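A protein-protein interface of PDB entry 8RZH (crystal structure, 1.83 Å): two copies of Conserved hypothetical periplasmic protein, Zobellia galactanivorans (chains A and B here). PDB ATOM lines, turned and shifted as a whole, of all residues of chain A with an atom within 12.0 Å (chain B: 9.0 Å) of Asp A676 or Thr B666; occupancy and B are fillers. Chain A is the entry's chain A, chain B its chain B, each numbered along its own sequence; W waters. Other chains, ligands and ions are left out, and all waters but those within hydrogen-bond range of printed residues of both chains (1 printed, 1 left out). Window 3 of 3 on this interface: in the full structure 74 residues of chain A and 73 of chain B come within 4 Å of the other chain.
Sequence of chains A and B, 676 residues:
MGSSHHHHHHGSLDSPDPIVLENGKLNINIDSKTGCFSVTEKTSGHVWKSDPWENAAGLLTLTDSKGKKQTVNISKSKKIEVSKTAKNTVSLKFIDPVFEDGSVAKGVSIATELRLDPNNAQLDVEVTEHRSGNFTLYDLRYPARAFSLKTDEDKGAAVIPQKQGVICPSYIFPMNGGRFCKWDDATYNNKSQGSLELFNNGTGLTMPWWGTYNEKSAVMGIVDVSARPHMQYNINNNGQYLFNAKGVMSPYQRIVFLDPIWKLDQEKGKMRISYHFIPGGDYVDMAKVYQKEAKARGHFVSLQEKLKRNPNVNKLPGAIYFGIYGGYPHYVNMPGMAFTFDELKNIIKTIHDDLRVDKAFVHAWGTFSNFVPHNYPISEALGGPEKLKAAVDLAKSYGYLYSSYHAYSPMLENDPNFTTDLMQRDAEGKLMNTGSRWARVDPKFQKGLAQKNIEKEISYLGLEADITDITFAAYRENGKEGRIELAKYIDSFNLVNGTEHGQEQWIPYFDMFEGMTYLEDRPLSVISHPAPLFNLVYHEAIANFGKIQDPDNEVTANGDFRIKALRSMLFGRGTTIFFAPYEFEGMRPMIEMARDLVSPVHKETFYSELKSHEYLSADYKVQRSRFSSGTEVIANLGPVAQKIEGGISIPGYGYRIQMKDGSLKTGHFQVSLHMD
N of His A674 sits at hydrogen-bond distance from O of His B668 (2.9 Å). The side-chain carboxylate of Asp A676 is in hydrogen-bond range of the side-chain hydroxyl of Thr B666 (2.6 Å).
The side-chain hydroxyl (OH) of Tyr B655 is in hydrogen-bond range of the backbone carbonyl oxygen (O) of Thr B666, 3.5 Å away. N of Phe B669 lies within hydrogen-bond range of O of Tyr B653 (3.0 Å). N of Tyr B655 is in hydrogen-bond range of O of Gly B667 (3.0 Å). A ring nitrogen (NE2) of His A674 lies within hydrogen-bond range of the side-chain carboxylate (OD1) of Asp A676 (2.7 Å).
Among the printed residues, merely in contact across the chains: Ser A672 with Phe B669, Leu A673 with Leu B597, Leu A673 with Tyr B655, Leu A673 with His B668, His A674 with Tyr B655, His A674 with Gly B667, Met A675 with Tyr B655, Met A675 with Thr B666 and Asp A676 with Gly B667.
Printed residues of chain B within 4 Å of Leu A673: Leu B597, Tyr B655 and His B668. Printed residues of chain B within 4 Å of Met A675: Tyr B655 and Thr B666. Of the printed residues of chain A, Leu B597 touches Leu A673. Tyr B653 touches none of the printed residues of chain A. Of chain A, only Leu A673, His A674 and Met A675 come within 4 Å of Tyr B655. No residue of chain A comes within 4 Å of Arg B656. No residue of chain A comes within 4 Å of Ile B657. Thr B666 touches two residues of chain A. The nearest residue of chain A that does not touch Thr B666 is His A674 (4.3 Å). The nearest printed residue of chain A that does not touch Phe B669 is Leu A673 (4.01 Å).
Of the 20 printed residues of chain B, 6 touch a printed residue of chain A. Hydrophobic or aromatic side chains of chain B that line the printed part of chain A: Leu B597, Tyr B655, His B668 and Phe B669. Hydrophobic or aromatic side chains of chain A that line the printed part of chain B: Leu A673, His A674 and Met A675. Among the printed residues, 11 pairs touch across the chains.
No position is printed for both chains.
Water W1 bridges the chain-end carboxylate of Asp A676 and the backbone NH of Thr B666.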
ATOM      1  N   SER A 672      11.800  12.427 -24.253  1.00  0.00           N
ATOM      2  CA  SER A 672      10.990  11.745 -25.242  1.00  0.00           C
ATOM      3  C   SER A 672       9.672  12.484 -25.410  1.00  0.00           C
ATOM      4  O   SER A 672       9.308  13.360 -24.616  1.00  0.00           O
ATOM      5  CB  SER A 672      10.745  10.270 -24.874  1.00  0.00           C
ATOM      6  OG  SER A 672      10.181  10.166 -23.584  1.00  0.00           O
ATOM      7  N   LEU A 673       8.953  12.091 -26.446  1.00  0.00           N
ATOM      8  CA  LEU A 673       7.708  12.743 -26.826  1.00  0.00           C
ATOM      9  C   LEU A 673       6.607  11.702 -26.742  1.00  0.00           C
ATOM     10  O   LEU A 673       6.603  10.760 -27.522  1.00  0.00           O
ATOM     11  CB  LEU A 673       7.825  13.307 -28.249  1.00  0.00           C
ATOM     12  CG  LEU A 673       6.487  13.806 -28.792  1.00  0.00           C
ATOM     13  CD1 LEU A 673       6.000  14.985 -27.964  1.00  0.00           C
ATOM     14  CD2 LEU A 673       6.687  14.163 -30.303  1.00  0.00           C
ATOM     15  N   HIS A 674       5.691  11.861 -25.786  1.00  0.00           N
ATOM     16  CA  HIS A 674       4.499  11.037 -25.733  1.00  0.00           C
ATOM     17  C   HIS A 674       3.445  11.621 -26.661  1.00  0.00           C
ATOM     18  O   HIS A 674       3.125  12.806 -26.560  1.00  0.00           O
ATOM     19  CB  HIS A 674       3.920  11.000 -24.305  1.00  0.00           C
ATOM     20  CG  HIS A 674       2.563  10.374 -24.272  1.00  0.00           C
ATOM     21  ND1 HIS A 674       2.376   9.029 -24.522  1.00  0.00           N
ATOM     22  CD2 HIS A 674       1.329  10.913 -24.111  1.00  0.00           C
ATOM     23  CE1 HIS A 674       1.075   8.762 -24.503  1.00  0.00           C
ATOM     24  NE2 HIS A 674       0.420   9.888 -24.248  1.00  0.00           N
ATOM     25  N   MET A 675       2.900  10.803 -27.540  1.00  0.00           N
ATOM     26  CA  MET A 675       1.818  11.218 -28.418  1.00  0.00           C
ATOM     27  C   MET A 675       0.661  10.259 -28.194  1.00  0.00           C
ATOM     28  O   MET A 675       0.829   9.050 -28.367  1.00  0.00           O
ATOM     29  CB  MET A 675       2.278  11.203 -29.885  1.00  0.00           C
ATOM     30  CG  MET A 675       3.567  12.008 -30.119  1.00  0.00           C
ATOM     31  SD  MET A 675       4.047  12.003 -31.888  1.00  0.00           S
ATOM     32  CE  MET A 675       3.025  13.388 -32.449  1.00  0.00           C
ATOM     33  N   ASP A 676      -0.493  10.795 -27.790  1.00  0.00           N
ATOM     34  CA  ASP A 676      -1.718   9.997 -27.595  1.00  0.00           C
ATOM     35  C   ASP A 676      -2.215   9.410 -28.886  1.00  0.00           C
ATOM     36  O   ASP A 676      -2.935   8.399 -28.852  1.00  0.00           O
ATOM     37  CB  ASP A 676      -2.851  10.822 -26.971  1.00  0.00           C
ATOM     38  CG  ASP A 676      -2.547  11.241 -25.560  1.00  0.00           C
ATOM     39  OD1 ASP A 676      -2.139  10.345 -24.791  1.00  0.00           O
ATOM     40  OD2 ASP A 676      -2.660  12.455 -25.216  1.00  0.00           O
ATOM     41  OXT ASP A 676      -1.928   9.929 -29.975  1.00  0.00           O
ATOM     42  N   LEU B 597       6.213  15.773 -34.455  1.00  0.00           N
ATOM     43  CA  LEU B 597       5.331  16.763 -33.835  1.00  0.00           C
ATOM     44  C   LEU B 597       5.267  18.073 -34.612  1.00  0.00           C
ATOM     45  O   LEU B 597       4.173  18.534 -34.977  1.00  0.00           O
ATOM     46  CB  LEU B 597       5.799  17.050 -32.405  1.00  0.00           C
ATOM     47  CG  LEU B 597       5.035  18.145 -31.656  1.00  0.00           C
ATOM     48  CD1 LEU B 597       3.634  17.669 -31.450  1.00  0.00           C
ATOM     49  CD2 LEU B 597       5.754  18.470 -30.325  1.00  0.00           C
ATOM     50  N   ILE B 634      -2.719  24.580 -29.106  1.00  0.00           N
ATOM     51  CA  ILE B 634      -2.637  24.951 -27.692  1.00  0.00           C
ATOM     52  C   ILE B 634      -1.385  24.293 -27.126  1.00  0.00           C
ATOM     53  O   ILE B 634      -1.155  23.102 -27.360  1.00  0.00           O
ATOM     54  CB  ILE B 634      -3.877  24.515 -26.895  1.00  0.00           C
ATOM     55  CG1 ILE B 634      -5.146  25.155 -27.516  1.00  0.00           C
ATOM     56  CG2 ILE B 634      -3.678  24.878 -25.393  1.00  0.00           C
ATOM     57  CD1 ILE B 634      -6.473  24.716 -26.827  1.00  0.00           C
ATOM     58  N   ILE B 648     -10.567  21.454 -19.598  1.00  0.00           N
ATOM     59  CA  ILE B 648      -9.561  20.733 -20.370  1.00  0.00           C
ATOM     60  C   ILE B 648      -8.213  20.976 -19.724  1.00  0.00           C
ATOM     61  O   ILE B 648      -7.871  22.116 -19.398  1.00  0.00           O
ATOM     62  CB  ILE B 648      -9.576  21.204 -21.836  1.00  0.00           C
ATOM     63  CG1 ILE B 648     -10.825  20.671 -22.558  1.00  0.00           C
ATOM     64  CG2 ILE B 648      -8.326  20.758 -22.607  1.00  0.00           C
ATOM     65  CD1 ILE B 648     -10.923  21.170 -23.994  1.00  0.00           C
ATOM     66  N   SER B 649      -7.442  19.919 -19.555  1.00  0.00           N
ATOM     67  CA  SER B 649      -6.122  20.035 -18.951  1.00  0.00           C
ATOM     68  C   SER B 649      -5.043  19.925 -20.037  1.00  0.00           C
ATOM     69  O   SER B 649      -5.099  19.021 -20.879  1.00  0.00           O
ATOM     70  CB  SER B 649      -5.958  18.946 -17.879  1.00  0.00           C
ATOM     71  OG  SER B 649      -4.702  19.053 -17.235  1.00  0.00           O
ATOM     72  N   ILE B 650      -4.077  20.836 -20.024  1.00  0.00           N
ATOM     73  CA  ILE B 650      -2.918  20.763 -20.911  1.00  0.00           C
ATOM     74  C   ILE B 650      -1.739  20.340 -20.044  1.00  0.00           C
ATOM     75  O   ILE B 650      -1.365  21.087 -19.122  1.00  0.00           O
ATOM     76  CB  ILE B 650      -2.601  22.094 -21.623  1.00  0.00           C
ATOM     77  CG1 ILE B 650      -3.837  22.787 -22.208  1.00  0.00           C
ATOM     78  CG2 ILE B 650      -1.597  21.872 -22.766  1.00  0.00           C
ATOM     79  CD1 ILE B 650      -4.591  21.922 -23.230  1.00  0.00           C
ATOM     80  N   PRO B 651      -1.109  19.193 -20.317  1.00  0.00           N
ATOM     81  CA  PRO B 651       0.046  18.762 -19.520  1.00  0.00           C
ATOM     82  C   PRO B 651       1.199  19.759 -19.558  1.00  0.00           C
ATOM     83  O   PRO B 651       1.390  20.516 -20.520  1.00  0.00           O
ATOM     84  CB  PRO B 651       0.476  17.442 -20.206  1.00  0.00           C
ATOM     85  CG  PRO B 651      -0.800  16.998 -21.004  1.00  0.00           C
ATOM     86  CD  PRO B 651      -1.330  18.306 -21.488  1.00  0.00           C
ATOM     87  N   TYR B 653       4.682  20.961 -20.521  1.00  0.00           N
ATOM     88  CA  TYR B 653       5.377  20.783 -21.807  1.00  0.00           C
ATOM     89  C   TYR B 653       4.522  19.943 -22.739  1.00  0.00           C
ATOM     90  O   TYR B 653       5.007  19.029 -23.407  1.00  0.00           O
ATOM     91  CB  TYR B 653       6.761  20.161 -21.607  1.00  0.00           C
ATOM     92  CG  TYR B 653       7.597  20.996 -20.628  1.00  0.00           C
ATOM     93  CD1 TYR B 653       7.906  22.341 -20.922  1.00  0.00           C
ATOM     94  CD2 TYR B 653       8.021  20.465 -19.397  1.00  0.00           C
ATOM     95  CE1 TYR B 653       8.656  23.132 -20.018  1.00  0.00           C
ATOM     96  CE2 TYR B 653       8.767  21.267 -18.488  1.00  0.00           C
ATOM     97  CZ  TYR B 653       9.060  22.586 -18.802  1.00  0.00           C
ATOM     98  OH  TYR B 653       9.783  23.401 -17.890  1.00  0.00           O
ATOM     99  N   GLY B 654       3.227  20.282 -22.795  1.00  0.00           N
ATOM    100  CA  GLY B 654       2.245  19.484 -23.496  1.00  0.00           C
ATOM    101  C   GLY B 654       1.509  20.315 -24.534  1.00  0.00           C
ATOM    102  O   GLY B 654       1.675  21.538 -24.628  1.00  0.00           O
ATOM    103  N   TYR B 655       0.697  19.629 -25.326  1.00  0.00           N
ATOM    104  CA  TYR B 655       0.030  20.313 -26.432  1.00  0.00           C
ATOM    105  C   TYR B 655      -1.317  19.642 -26.702  1.00  0.00           C
ATOM    106  O   TYR B 655      -1.574  18.482 -26.332  1.00  0.00           O
ATOM    107  CB  TYR B 655       0.913  20.310 -27.708  1.00  0.00           C
ATOM    108  CG  TYR B 655       1.226  18.887 -28.144  1.00  0.00           C
ATOM    109  CD1 TYR B 655       2.340  18.210 -27.619  1.00  0.00           C
ATOM    110  CD2 TYR B 655       0.396  18.206 -29.036  1.00  0.00           C
ATOM    111  CE1 TYR B 655       2.621  16.899 -27.997  1.00  0.00           C
ATOM    112  CE2 TYR B 655       0.668  16.893 -29.398  1.00  0.00           C
ATOM    113  CZ  TYR B 655       1.771  16.253 -28.865  1.00  0.00           C
ATOM    114  OH  TYR B 655       2.022  14.936 -29.215  1.00  0.00           O
ATOM    115  N   ARG B 656      -2.192  20.419 -27.335  1.00  0.00           N
ATOM    116  CA  ARG B 656      -3.493  19.947 -27.781  1.00  0.00           C
ATOM    117  C   ARG B 656      -3.743  20.675 -29.099  1.00  0.00           C
ATOM    118  O   ARG B 656      -3.940  21.887 -29.090  1.00  0.00           O
ATOM    119  CB  ARG B 656      -4.561  20.274 -26.736  1.00  0.00           C
ATOM    120  CG  ARG B 656      -5.965  19.949 -27.173  1.00  0.00           C
ATOM    121  CD  ARG B 656      -6.942  20.283 -26.035  1.00  0.00           C
ATOM    122  NE  ARG B 656      -8.248  19.711 -26.302  1.00  0.00           N
ATOM    123  CZ  ARG B 656      -8.671  18.529 -25.827  1.00  0.00           C
ATOM    124  NH1 ARG B 656      -7.912  17.765 -25.038  1.00  0.00           N
ATOM    125  NH2 ARG B 656      -9.880  18.110 -26.145  1.00  0.00           N
ATOM    126  N   ILE B 657      -3.687  19.968 -30.223  1.00  0.00           N
ATOM    127  CA  ILE B 657      -3.636  20.625 -31.539  1.00  0.00           C
ATOM    128  C   ILE B 657      -4.771  20.082 -32.394  1.00  0.00           C
ATOM    129  O   ILE B 657      -4.881  18.866 -32.624  1.00  0.00           O
ATOM    130  CB  ILE B 657      -2.275  20.423 -32.223  1.00  0.00           C
ATOM    131  CG1 ILE B 657      -1.126  20.991 -31.355  1.00  0.00           C
ATOM    132  CG2 ILE B 657      -2.345  20.975 -33.667  1.00  0.00           C
ATOM    133  CD1 ILE B 657       0.300  20.644 -31.870  1.00  0.00           C
ATOM    134  N   GLN B 658      -5.637  20.973 -32.850  1.00  0.00           N
ATOM    135  CA  GLN B 658      -6.746  20.574 -33.693  1.00  0.00           C
ATOM    136  C   GLN B 658      -6.301  20.802 -35.140  1.00  0.00           C
ATOM    137  O   GLN B 658      -5.977  21.930 -35.513  1.00  0.00           O
ATOM    138  CB  GLN B 658      -8.000  21.370 -33.330  1.00  0.00           C
ATOM    139  CG  GLN B 658      -9.103  21.219 -34.337  1.00  0.00           C
ATOM    140  CD  GLN B 658      -9.756  19.863 -34.303  1.00  0.00           C
ATOM    141  OE1 GLN B 658     -10.545  19.573 -33.404  1.00  0.00           O
ATOM    142  NE2 GLN B 658      -9.455  19.025 -35.303  1.00  0.00           N
ATOM    143  N   MET B 659      -6.200  19.719 -35.913  1.00  0.00           N
ATOM    144  CA  MET B 659      -5.767  19.804 -37.304  1.00  0.00           C
ATOM    145  C   MET B 659      -6.957  20.004 -38.230  1.00  0.00           C
ATOM    146  O   MET B 659      -8.094  19.694 -37.897  1.00  0.00           O
ATOM    147  CB  MET B 659      -5.024  18.538 -37.743  1.00  0.00           C
ATOM    148  CG  MET B 659      -3.826  18.211 -36.823  1.00  0.00           C
ATOM    149  SD  MET B 659      -2.464  19.407 -36.969  1.00  0.00           S
ATOM    150  CE  MET B 659      -1.866  19.113 -38.634  1.00  0.00           C
ATOM    151  N   SER B 663      -8.382  15.623 -36.916  1.00  0.00           N
ATOM    152  CA  SER B 663      -7.676  14.896 -35.881  1.00  0.00           C
ATOM    153  C   SER B 663      -7.274  15.860 -34.776  1.00  0.00           C
ATOM    154  O   SER B 663      -7.044  17.052 -35.012  1.00  0.00           O
ATOM    155  CB  SER B 663      -6.451  14.176 -36.467  1.00  0.00           C
ATOM    156  OG  SER B 663      -5.492  15.086 -36.933  1.00  0.00           O
ATOM    157  N   LEU B 664      -7.200  15.339 -33.544  1.00  0.00           N
ATOM    158  CA  LEU B 664      -6.766  16.134 -32.401  1.00  0.00           C
ATOM    159  C   LEU B 664      -5.472  15.516 -31.876  1.00  0.00           C
ATOM    160  O   LEU B 664      -5.482  14.367 -31.415  1.00  0.00           O
ATOM    161  CB  LEU B 664      -7.865  16.123 -31.338  1.00  0.00           C
ATOM    162  CG  LEU B 664      -7.573  16.915 -30.074  1.00  0.00           C
ATOM    163  CD1 LEU B 664      -7.710  18.402 -30.392  1.00  0.00           C
ATOM    164  CD2 LEU B 664      -8.565  16.464 -29.009  1.00  0.00           C
ATOM    165  N   LYS B 665      -4.362  16.228 -31.982  1.00  0.00           N
ATOM    166  CA  LYS B 665      -3.081  15.686 -31.524  1.00  0.00           C
ATOM    167  C   LYS B 665      -2.878  16.129 -30.082  1.00  0.00           C
ATOM    168  O   LYS B 665      -2.922  17.327 -29.805  1.00  0.00           O
ATOM    169  CB  LYS B 665      -1.944  16.178 -32.417  1.00  0.00           C
ATOM    170  CG  LYS B 665      -2.255  15.770 -33.871  1.00  0.00           C
ATOM    171  CD  LYS B 665      -1.049  15.698 -34.749  1.00  0.00           C
ATOM    172  CE  LYS B 665      -0.669  17.072 -35.211  1.00  0.00           C
ATOM    173  NZ  LYS B 665       0.008  17.056 -36.561  1.00  0.00           N
ATOM    174  N   THR B 666      -2.715  15.177 -29.171  1.00  0.00           N
ATOM    175  CA  THR B 666      -2.406  15.505 -27.788  1.00  0.00           C
ATOM    176  C   THR B 666      -1.177  14.715 -27.333  1.00  0.00           C
ATOM    177  O   THR B 666      -0.898  13.614 -27.836  1.00  0.00           O
ATOM    178  CB  THR B 666      -3.596  15.212 -26.847  1.00  0.00           C
ATOM    179  OG1 THR B 666      -4.026  13.849 -26.981  1.00  0.00           O
ATOM    180  CG2 THR B 666      -4.804  16.129 -27.207  1.00  0.00           C
ATOM    181  N   GLY B 667      -0.455  15.270 -26.369  1.00  0.00           N
ATOM    182  CA  GLY B 667       0.778  14.627 -25.948  1.00  0.00           C
ATOM    183  C   GLY B 667       1.572  15.592 -25.094  1.00  0.00           C
ATOM    184  O   GLY B 667       1.104  16.690 -24.780  1.00  0.00           O
ATOM    185  N   HIS B 668       2.800  15.182 -24.772  1.00  0.00           N
ATOM    186  CA  HIS B 668       3.670  16.021 -23.965  1.00  0.00           C
ATOM    187  C   HIS B 668       5.067  15.412 -23.963  1.00  0.00           C
ATOM    188  O   HIS B 668       5.253  14.221 -24.243  1.00  0.00           O
ATOM    189  CB  HIS B 668       3.152  16.140 -22.532  1.00  0.00           C
ATOM    190  CG  HIS B 668       3.138  14.819 -21.815  1.00  0.00           C
ATOM    191  ND1 HIS B 668       2.064  13.957 -21.852  1.00  0.00           N
ATOM    192  CD2 HIS B 668       4.088  14.209 -21.054  1.00  0.00           C
ATOM    193  CE1 HIS B 668       2.337  12.878 -21.134  1.00  0.00           C
ATOM    194  NE2 HIS B 668       3.563  12.996 -20.654  1.00  0.00           N
ATOM    195  N   PHE B 669       6.038  16.258 -23.659  1.00  0.00           N
ATOM    196  CA  PHE B 669       7.423  15.823 -23.527  1.00  0.00           C
ATOM    197  C   PHE B 669       7.643  15.278 -22.136  1.00  0.00           C
ATOM    198  O   PHE B 669       7.033  15.737 -21.171  1.00  0.00           O
ATOM    199  CB  PHE B 669       8.380  17.002 -23.773  1.00  0.00           C
ATOM    200  CG  PHE B 669       8.449  17.425 -25.230  1.00  0.00           C
ATOM    201  CD1 PHE B 669       9.273  16.751 -26.119  1.00  0.00           C
ATOM    202  CD2 PHE B 669       7.665  18.477 -25.706  1.00  0.00           C
ATOM    203  CE1 PHE B 669       9.357  17.129 -27.461  1.00  0.00           C
ATOM    204  CE2 PHE B 669       7.729  18.862 -27.064  1.00  0.00           C
ATOM    205  CZ  PHE B 669       8.582  18.192 -27.934  1.00  0.00           C
HETATM  206  O   HOH W   1      -2.594  12.515 -30.480  1.00  0.00           O
